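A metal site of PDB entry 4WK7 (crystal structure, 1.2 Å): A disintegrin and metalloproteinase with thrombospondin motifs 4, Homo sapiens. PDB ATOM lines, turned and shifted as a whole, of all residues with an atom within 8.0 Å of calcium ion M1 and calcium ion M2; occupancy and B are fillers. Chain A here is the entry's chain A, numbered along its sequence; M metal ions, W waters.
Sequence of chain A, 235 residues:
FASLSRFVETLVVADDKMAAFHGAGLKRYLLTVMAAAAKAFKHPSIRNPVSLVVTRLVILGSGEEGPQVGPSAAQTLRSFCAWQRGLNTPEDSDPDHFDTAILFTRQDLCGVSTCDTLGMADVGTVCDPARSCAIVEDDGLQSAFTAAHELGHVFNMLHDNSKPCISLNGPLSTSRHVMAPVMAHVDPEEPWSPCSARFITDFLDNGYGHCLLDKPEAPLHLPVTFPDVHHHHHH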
ATOM      1  N   PHE A   7     -27.895 -17.713  25.700  1.00  0.00           N
ATOM      2  CA  PHE A   7     -27.391 -17.168  26.961  1.00  0.00           C
ATOM      3  C   PHE A   7     -28.508 -16.470  27.704  1.00  0.00           C
ATOM      4  O   PHE A   7     -29.207 -15.632  27.143  1.00  0.00           O
ATOM      5  CB  PHE A   7     -26.259 -16.167  26.681  1.00  0.00           C
ATOM      6  CG  PHE A   7     -25.174 -16.718  25.804  1.00  0.00           C
ATOM      7  CD1 PHE A   7     -24.124 -17.442  26.345  1.00  0.00           C
ATOM      8  CD2 PHE A   7     -25.214 -16.524  24.424  1.00  0.00           C
ATOM      9  CE1 PHE A   7     -23.127 -17.956  25.527  1.00  0.00           C
ATOM     10  CE2 PHE A   7     -24.212 -17.028  23.616  1.00  0.00           C
ATOM     11  CZ  PHE A   7     -23.171 -17.744  24.163  1.00  0.00           C
ATOM     12  N   VAL A   8     -28.691 -16.835  28.973  1.00  0.00           N
ATOM     13  CA  VAL A   8     -29.664 -16.173  29.825  1.00  0.00           C
ATOM     14  C   VAL A   8     -28.927 -15.218  30.751  1.00  0.00           C
ATOM     15  O   VAL A   8     -28.245 -15.650  31.681  1.00  0.00           O
ATOM     16  CB  VAL A   8     -30.466 -17.167  30.680  1.00  0.00           C
ATOM     17  CG1 VAL A   8     -31.644 -16.473  31.343  1.00  0.00           C
ATOM     18  CG2 VAL A   8     -30.961 -18.330  29.831  1.00  0.00           C
ATOM     19  N   GLU A   9     -29.036 -13.915  30.463  1.00  0.00           N
ATOM     20  CA  GLU A   9     -28.394 -12.902  31.288  1.00  0.00           C
ATOM     21  C   GLU A   9     -29.223 -12.728  32.550  1.00  0.00           C
ATOM     22  O   GLU A   9     -30.366 -12.275  32.506  1.00  0.00           O
ATOM     23  CB  GLU A   9     -28.269 -11.592  30.498  1.00  0.00           C
ATOM     24  CG  GLU A   9     -27.371 -11.737  29.277  1.00  0.00           C
ATOM     25  CD  GLU A   9     -27.439 -10.533  28.362  1.00  0.00           C
ATOM     26  OE1 GLU A   9     -28.493 -10.331  27.718  1.00  0.00           O
ATOM     27  OE2 GLU A   9     -26.466  -9.767  28.269  1.00  0.00           O
ATOM     28  N   THR A  10     -28.660 -13.132  33.676  1.00  0.00           N
ATOM     29  CA  THR A  10     -29.446 -13.323  34.890  1.00  0.00           C
ATOM     30  C   THR A  10     -29.098 -12.321  35.983  1.00  0.00           C
ATOM     31  O   THR A  10     -27.929 -12.156  36.339  1.00  0.00           O
ATOM     32  CB  THR A  10     -29.261 -14.754  35.426  1.00  0.00           C
ATOM     33  OG1 THR A  10     -29.550 -15.688  34.386  1.00  0.00           O
ATOM     34  CG2 THR A  10     -30.164 -15.020  36.624  1.00  0.00           C
ATOM     35  N   THR A  55     -25.112 -12.033  35.486  1.00  0.00           N
ATOM     36  CA  THR A  55     -24.556 -10.767  35.001  1.00  0.00           C
ATOM     37  C   THR A  55     -24.702  -9.632  36.014  1.00  0.00           C
ATOM     38  O   THR A  55     -23.922  -8.683  35.975  1.00  0.00           O
ATOM     39  CB  THR A  55     -25.193 -10.360  33.661  1.00  0.00           C
ATOM     40  OG1 THR A  55     -26.620 -10.310  33.795  1.00  0.00           O
ATOM     41  CG2 THR A  55     -24.825 -11.352  32.580  1.00  0.00           C
ATOM     42  N   THR A  89     -33.216  -2.229  31.917  1.00  0.00           N
ATOM     43  CA  THR A  89     -33.185  -1.195  30.876  1.00  0.00           C
ATOM     44  C   THR A  89     -34.096  -1.637  29.727  1.00  0.00           C
ATOM     45  O   THR A  89     -34.402  -2.820  29.599  1.00  0.00           O
ATOM     46  CB  THR A  89     -31.772  -0.992  30.335  1.00  0.00           C
ATOM     47  OG1 THR A  89     -31.313  -2.197  29.699  1.00  0.00           O
ATOM     48  CG2 THR A  89     -30.810  -0.624  31.457  1.00  0.00           C
ATOM     49  N   GLU A  91     -33.528  -1.917  26.485  1.00  0.00           N
ATOM     50  CA  GLU A  91     -32.905  -2.626  25.364  1.00  0.00           C
ATOM     51  C   GLU A  91     -31.874  -3.652  25.807  1.00  0.00           C
ATOM     52  O   GLU A  91     -31.028  -3.378  26.661  1.00  0.00           O
ATOM     53  CB  GLU A  91     -32.261  -1.628  24.408  1.00  0.00           C
ATOM     54  CG  GLU A  91     -33.228  -0.609  23.817  1.00  0.00           C
ATOM     55  CD  GLU A  91     -34.310  -1.230  22.962  1.00  0.00           C
ATOM     56  OE1 GLU A  91     -34.143  -2.385  22.515  1.00  0.00           O
ATOM     57  OE2 GLU A  91     -35.345  -0.566  22.738  1.00  0.00           O
ATOM     58  N   ASP A  92     -31.928  -4.838  25.188  1.00  0.00           N
ATOM     59  CA  ASP A  92     -31.023  -5.939  25.525  1.00  0.00           C
ATOM     60  C   ASP A  92     -29.571  -5.633  25.146  1.00  0.00           C
ATOM     61  O   ASP A  92     -28.646  -6.206  25.709  1.00  0.00           O
ATOM     62  CB  ASP A  92     -31.505  -7.235  24.858  1.00  0.00           C
ATOM     63  CG  ASP A  92     -31.054  -8.502  25.573  1.00  0.00           C
ATOM     64  OD1 ASP A  92     -30.254  -8.466  26.531  1.00  0.00           O
ATOM     65  OD2 ASP A  92     -31.514  -9.587  25.161  1.00  0.00           O
ATOM     66  N   SER A  93     -29.356  -4.713  24.205  1.00  0.00           N
ATOM     67  CA  SER A  93     -27.991  -4.303  23.843  1.00  0.00           C
ATOM     68  C   SER A  93     -27.289  -3.448  24.901  1.00  0.00           C
ATOM     69  O   SER A  93     -26.073  -3.302  24.871  1.00  0.00           O
ATOM     70  CB  SER A  93     -27.989  -3.576  22.497  1.00  0.00           C
ATOM     71  OG  SER A  93     -28.809  -2.428  22.537  1.00  0.00           O
ATOM     72  N   ASP A  94     -28.055  -2.876  25.839  1.00  0.00           N
ATOM     73  CA  ASP A  94     -27.469  -2.179  26.979  1.00  0.00           C
ATOM     74  C   ASP A  94     -26.873  -3.233  27.919  1.00  0.00           C
ATOM     75  O   ASP A  94     -27.575  -4.178  28.276  1.00  0.00           O
ATOM     76  CB  ASP A  94     -28.554  -1.375  27.701  1.00  0.00           C
ATOM     77  CG  ASP A  94     -28.005  -0.507  28.821  1.00  0.00           C
ATOM     78  OD1 ASP A  94     -27.261  -1.017  29.681  1.00  0.00           O
ATOM     79  OD2 ASP A  94     -28.344   0.692  28.846  1.00  0.00           O
ATOM     80  N   PRO A  95     -25.599  -3.089  28.326  1.00  0.00           N
ATOM     81  CA  PRO A  95     -24.999  -4.149  29.156  1.00  0.00           C
ATOM     82  C   PRO A  95     -25.680  -4.363  30.515  1.00  0.00           C
ATOM     83  O   PRO A  95     -25.561  -5.457  31.076  1.00  0.00           O
ATOM     84  CB  PRO A  95     -23.556  -3.676  29.356  1.00  0.00           C
ATOM     85  CG  PRO A  95     -23.607  -2.207  29.141  1.00  0.00           C
ATOM     86  CD  PRO A  95     -24.654  -1.983  28.091  1.00  0.00           C
ATOM     87  N   ASP A  96     -26.402  -3.360  31.026  1.00  0.00           N
ATOM     88  CA  ASP A  96     -27.142  -3.503  32.286  1.00  0.00           C
ATOM     89  C   ASP A  96     -28.432  -4.306  32.126  1.00  0.00           C
ATOM     90  O   ASP A  96     -29.033  -4.703  33.133  1.00  0.00           O
ATOM     91  CB  ASP A  96     -27.500  -2.135  32.873  1.00  0.00           C
ATOM     92  CG  ASP A  96     -26.291  -1.344  33.320  1.00  0.00           C
ATOM     93  OD1 ASP A  96     -25.183  -1.909  33.435  1.00  0.00           O
ATOM     94  OD2 ASP A  96     -26.460  -0.135  33.584  1.00  0.00           O
ATOM     95  N   HIS A  97     -28.888  -4.530  30.899  1.00  0.00           N
ATOM     96  CA  HIS A  97     -30.118  -5.293  30.693  1.00  0.00           C
ATOM     97  C   HIS A  97     -29.928  -6.740  31.118  1.00  0.00           C
ATOM     98  O   HIS A  97     -28.856  -7.318  30.923  1.00  0.00           O
ATOM     99  CB  HIS A  97     -30.555  -5.263  29.228  1.00  0.00           C
ATOM    100  CG  HIS A  97     -31.890  -5.907  28.992  1.00  0.00           C
ATOM    101  ND1 HIS A  97     -33.075  -5.205  29.032  1.00  0.00           N
ATOM    102  CD2 HIS A  97     -32.230  -7.194  28.711  1.00  0.00           C
ATOM    103  CE1 HIS A  97     -34.084  -6.021  28.789  1.00  0.00           C
ATOM    104  NE2 HIS A  97     -33.597  -7.230  28.597  1.00  0.00           N
ATOM    105  N   PHE A  98     -30.974  -7.319  31.690  1.00  0.00           N
ATOM    106  CA  PHE A  98     -30.986  -8.738  32.043  1.00  0.00           C
ATOM    107  C   PHE A  98     -32.243  -9.410  31.507  1.00  0.00           C
ATOM    108  O   PHE A  98     -33.279  -8.760  31.317  1.00  0.00           O
ATOM    109  CB  PHE A  98     -30.831  -8.941  33.551  1.00  0.00           C
ATOM    110  CG  PHE A  98     -31.801  -8.155  34.377  1.00  0.00           C
ATOM    111  CD1 PHE A  98     -33.038  -8.687  34.729  1.00  0.00           C
ATOM    112  CD2 PHE A  98     -31.478  -6.870  34.823  1.00  0.00           C
ATOM    113  CE1 PHE A  98     -33.920  -7.958  35.494  1.00  0.00           C
ATOM    114  CE2 PHE A  98     -32.360  -6.141  35.588  1.00  0.00           C
ATOM    115  CZ  PHE A  98     -33.593  -6.681  35.925  1.00  0.00           C
ATOM    116  N   ASP A  99     -32.139 -10.704  31.253  1.00  0.00           N
ATOM    117  CA  ASP A  99     -33.221 -11.501  30.666  1.00  0.00           C
ATOM    118  C   ASP A  99     -34.120 -12.171  31.705  1.00  0.00           C
ATOM    119  O   ASP A  99     -35.259 -12.502  31.398  1.00  0.00           O
ATOM    120  CB  ASP A  99     -32.654 -12.595  29.770  1.00  0.00           C
ATOM    121  CG  ASP A  99     -31.790 -12.057  28.645  1.00  0.00           C
ATOM    122  OD1 ASP A  99     -32.186 -11.066  27.976  1.00  0.00           O
ATOM    123  OD2 ASP A  99     -30.713 -12.639  28.399  1.00  0.00           O
ATOM    124  N   THR A 100     -33.606 -12.425  32.900  1.00  0.00           N
ATOM    125  CA  THR A 100     -34.428 -13.031  33.944  1.00  0.00           C
ATOM    126  C   THR A 100     -33.931 -12.580  35.308  1.00  0.00           C
ATOM    127  O   THR A 100     -32.768 -12.175  35.441  1.00  0.00           O
ATOM    128  CB  THR A 100     -34.470 -14.572  33.820  1.00  0.00           C
ATOM    129  OG1 THR A 100     -35.677 -15.063  34.418  1.00  0.00           O
ATOM    130  CG2 THR A 100     -33.271 -15.240  34.461  1.00  0.00           C
ATOM    131  N   VAL A 126     -39.489 -16.179  29.690  1.00  0.00           N
ATOM    132  CA  VAL A 126     -38.070 -15.825  29.787  1.00  0.00           C
ATOM    133  C   VAL A 126     -37.697 -14.545  29.028  1.00  0.00           C
ATOM    134  O   VAL A 126     -36.807 -13.813  29.481  1.00  0.00           O
ATOM    135  CB  VAL A 126     -37.151 -17.009  29.362  1.00  0.00           C
ATOM    136  CG1 VAL A 126     -37.071 -17.155  27.851  1.00  0.00           C
ATOM    137  CG2 VAL A 126     -35.747 -16.830  29.950  1.00  0.00           C
ATOM    138  N   CYS A 127     -38.363 -14.251  27.921  1.00  0.00           N
ATOM    139  CA  CYS A 127     -38.040 -13.034  27.163  1.00  0.00           C
ATOM    140  C   CYS A 127     -39.103 -11.957  27.255  1.00  0.00           C
ATOM    141  O   CYS A 127     -39.211 -11.113  26.368  1.00  0.00           O
ATOM    142  CB  CYS A 127     -37.719 -13.395  25.707  1.00  0.00           C
ATOM    143  SG  CYS A 127     -36.144 -14.264  25.571  1.00  0.00           S
ATOM    144  N   GLY A 209     -37.491 -17.495  22.808  1.00  0.00           N
ATOM    145  CA  GLY A 209     -36.156 -17.232  23.341  1.00  0.00           C
ATOM    146  C   GLY A 209     -35.350 -16.223  22.533  1.00  0.00           C
ATOM    147  O   GLY A 209     -34.124 -16.270  22.514  1.00  0.00           O
ATOM    148  N   HIS A 210     -36.051 -15.301  21.873  1.00  0.00           N
ATOM    149  CA  HIS A 210     -35.426 -14.305  21.000  1.00  0.00           C
ATOM    150  C   HIS A 210     -34.465 -13.350  21.713  1.00  0.00           C
ATOM    151  O   HIS A 210     -33.607 -12.743  21.073  1.00  0.00           O
ATOM    152  CB  HIS A 210     -36.505 -13.486  20.261  1.00  0.00           C
ATOM    153  CG  HIS A 210     -37.445 -12.770  21.179  1.00  0.00           C
ATOM    154  ND1 HIS A 210     -37.150 -11.554  21.755  1.00  0.00           N
ATOM    155  CD2 HIS A 210     -38.675 -13.114  21.640  1.00  0.00           C
ATOM    156  CE1 HIS A 210     -38.152 -11.175  22.516  1.00  0.00           C
ATOM    157  NE2 HIS A 210     -39.094 -12.103  22.470  1.00  0.00           N
ATOM    158  N   CYS A 211     -34.602 -13.223  23.033  1.00  0.00           N
ATOM    159  CA  CYS A 211     -33.697 -12.385  23.842  1.00  0.00           C
ATOM    160  C   CYS A 211     -32.475 -13.147  24.365  1.00  0.00           C
ATOM    161  O   CYS A 211     -31.677 -12.579  25.111  1.00  0.00           O
ATOM    162  CB  CYS A 211     -34.469 -11.793  25.023  1.00  0.00           C
ATOM    163  SG  CYS A 211     -34.805 -12.954  26.363  1.00  0.00           S
ATOM    164  N   LEU A 212     -32.312 -14.411  23.982  1.00  0.00           N
ATOM    165  CA  LEU A 212     -31.242 -15.244  24.513  1.00  0.00           C
ATOM    166  C   LEU A 212     -30.085 -15.424  23.529  1.00  0.00           C
ATOM    167  O   LEU A 212     -29.215 -16.267  23.734  1.00  0.00           O
ATOM    168  CB  LEU A 212     -31.794 -16.619  24.903  1.00  0.00           C
ATOM    169  CG  LEU A 212     -32.990 -16.620  25.859  1.00  0.00           C
ATOM    170  CD1 LEU A 212     -33.464 -18.036  26.136  1.00  0.00           C
ATOM    171  CD2 LEU A 212     -32.662 -15.898  27.163  1.00  0.00           C
ATOM    172  N   LEU A 213     -30.058 -14.621  22.470  1.00  0.00           N
ATOM    173  CA  LEU A 213     -29.070 -14.810  21.403  1.00  0.00           C
ATOM    174  C   LEU A 213     -27.824 -13.949  21.561  1.00  0.00           C
ATOM    175  O   LEU A 213     -26.793 -14.268  20.976  1.00  0.00           O
ATOM    176  CB  LEU A 213     -29.717 -14.542  20.033  1.00  0.00           C
ATOM    177  CG  LEU A 213     -31.048 -15.241  19.754  1.00  0.00           C
ATOM    178  CD1 LEU A 213     -31.603 -14.798  18.401  1.00  0.00           C
ATOM    179  CD2 LEU A 213     -30.884 -16.752  19.798  1.00  0.00           C
ATOM    180  N   ASP A 214     -27.898 -12.861  22.334  1.00  0.00           N
ATOM    181  CA  ASP A 214     -26.727 -12.013  22.561  1.00  0.00           C
ATOM    182  C   ASP A 214     -25.857 -12.541  23.696  1.00  0.00           C
ATOM    183  O   ASP A 214     -26.348 -13.032  24.708  1.00  0.00           O
ATOM    184  CB  ASP A 214     -27.126 -10.529  22.782  1.00  0.00           C
ATOM    185  CG  ASP A 214     -28.018 -10.302  23.993  1.00  0.00           C
ATOM    186  OD1 ASP A 214     -28.916 -11.128  24.272  1.00  0.00           O
ATOM    187  OD2 ASP A 214     -27.833  -9.266  24.658  1.00  0.00           O
ATOM    188  N   LYS A 215     -24.538 -12.470  23.511  1.00  0.00           N
ATOM    189  CA  LYS A 215     -23.583 -13.021  24.472  1.00  0.00           C
ATOM    190  C   LYS A 215     -23.156 -11.940  25.462  1.00  0.00           C
ATOM    191  O   LYS A 215     -22.688 -10.879  25.037  1.00  0.00           O
ATOM    192  CB  LYS A 215     -22.372 -13.593  23.738  1.00  0.00           C
ATOM    193  CG  LYS A 215     -21.501 -14.517  24.576  1.00  0.00           C
ATOM    194  CD  LYS A 215     -20.475 -15.236  23.721  1.00  0.00           C
ATOM    195  CE  LYS A 215     -19.721 -16.293  24.513  1.00  0.00           C
ATOM    196  NZ  LYS A 215     -18.814 -17.109  23.654  1.00  0.00           N
ATOM    197  N   PRO A 216     -23.331 -12.179  26.772  1.00  0.00           N
ATOM    198  CA  PRO A 216     -23.003 -11.145  27.762  1.00  0.00           C
ATOM    199  C   PRO A 216     -21.505 -10.844  27.840  1.00  0.00           C
ATOM    200  O   PRO A 216     -20.687 -11.750  27.716  1.00  0.00           O
ATOM    201  CB  PRO A 216     -23.493 -11.738  29.096  1.00  0.00           C
ATOM    202  CG  PRO A 216     -23.569 -13.196  28.858  1.00  0.00           C
ATOM    203  CD  PRO A 216     -23.848 -13.410  27.402  1.00  0.00           C
ATOM    204  N   GLU A 217     -21.182  -9.572  28.071  1.00  0.00           N
ATOM    205  CA  GLU A 217     -19.797  -9.091  28.024  1.00  0.00           C
ATOM    206  C   GLU A 217     -19.004  -9.389  29.299  1.00  0.00           C
ATOM    207  O   GLU A 217     -17.799  -9.623  29.241  1.00  0.00           O
ATOM    208  CB  GLU A 217     -19.782  -7.583  27.772  1.00  0.00           C
HETATM  209 CA    CA M   1     -30.201 -11.270  26.374  1.00  0.00          CA
HETATM  210 CA    CA M   2     -27.826  -8.231  26.680  1.00  0.00          CA
HETATM  211  O   HOH W   1     -28.640 -13.123  26.265  1.00  0.00           O
HETATM  212  O   HOH W   2     -27.532  -6.867  28.551  1.00  0.00           O
HETATM  213  O   HOH W   3     -25.674  -7.583  25.998  1.00  0.00           O
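Water W1 lies within hydrogen-bond range of O of Phe 7 (2.7 Å) and O of Asp 214 (2.8 Å).
Five residues have an atom within 4 Å of calcium ion M1: Glu 9, Asp 92, Asp 99, Cys 211 and Asp 214. The nearest printed residue that does not touch calcium ion M1 is Leu 212 (4.5 Å).
The side-chain sulfur (SG) of Cys 211 forms a disulfide with the side-chain sulfur (SG) of Cys 127. N of Thr 100 is in hydrogen-bond range of O of Glu 9 (3.3 Å).
O of Cys 211 is bound to calcium ion M1 (2.3 Å). OE1 of Glu 9 is bound to calcium ion M1 (2.4 Å). Calcium ion M1 is bound by water W1 (2.4 Å). Calcium ion M1 is bound by OD2 of Asp 92 (2.5 Å). OD1 of Asp 214 binds calcium ion M1 (2.5 Å). OD2 of Asp 99 binds calcium ion M1 (2.5 Å). OD1 of Asp 99 is bound to calcium ion M1 (2.6 Å). The side-chain carboxylate (OD1) of Asp 92 is bound to calcium ion M1 (2.8 Å). Calcium ion M1 has eight donor atoms within binding distance.
Calcium ion M2 is bound by OD2 of Asp 214 (2.3 Å), water W2 (2.3 Å), water W3 (2.3 Å), O of Asp 92 (2.4 Å), OE1 of Glu 9 (2.4 Å), OD1 of Asp 92 (2.4 Å) and OE2 of Glu 9 (2.6 Å).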
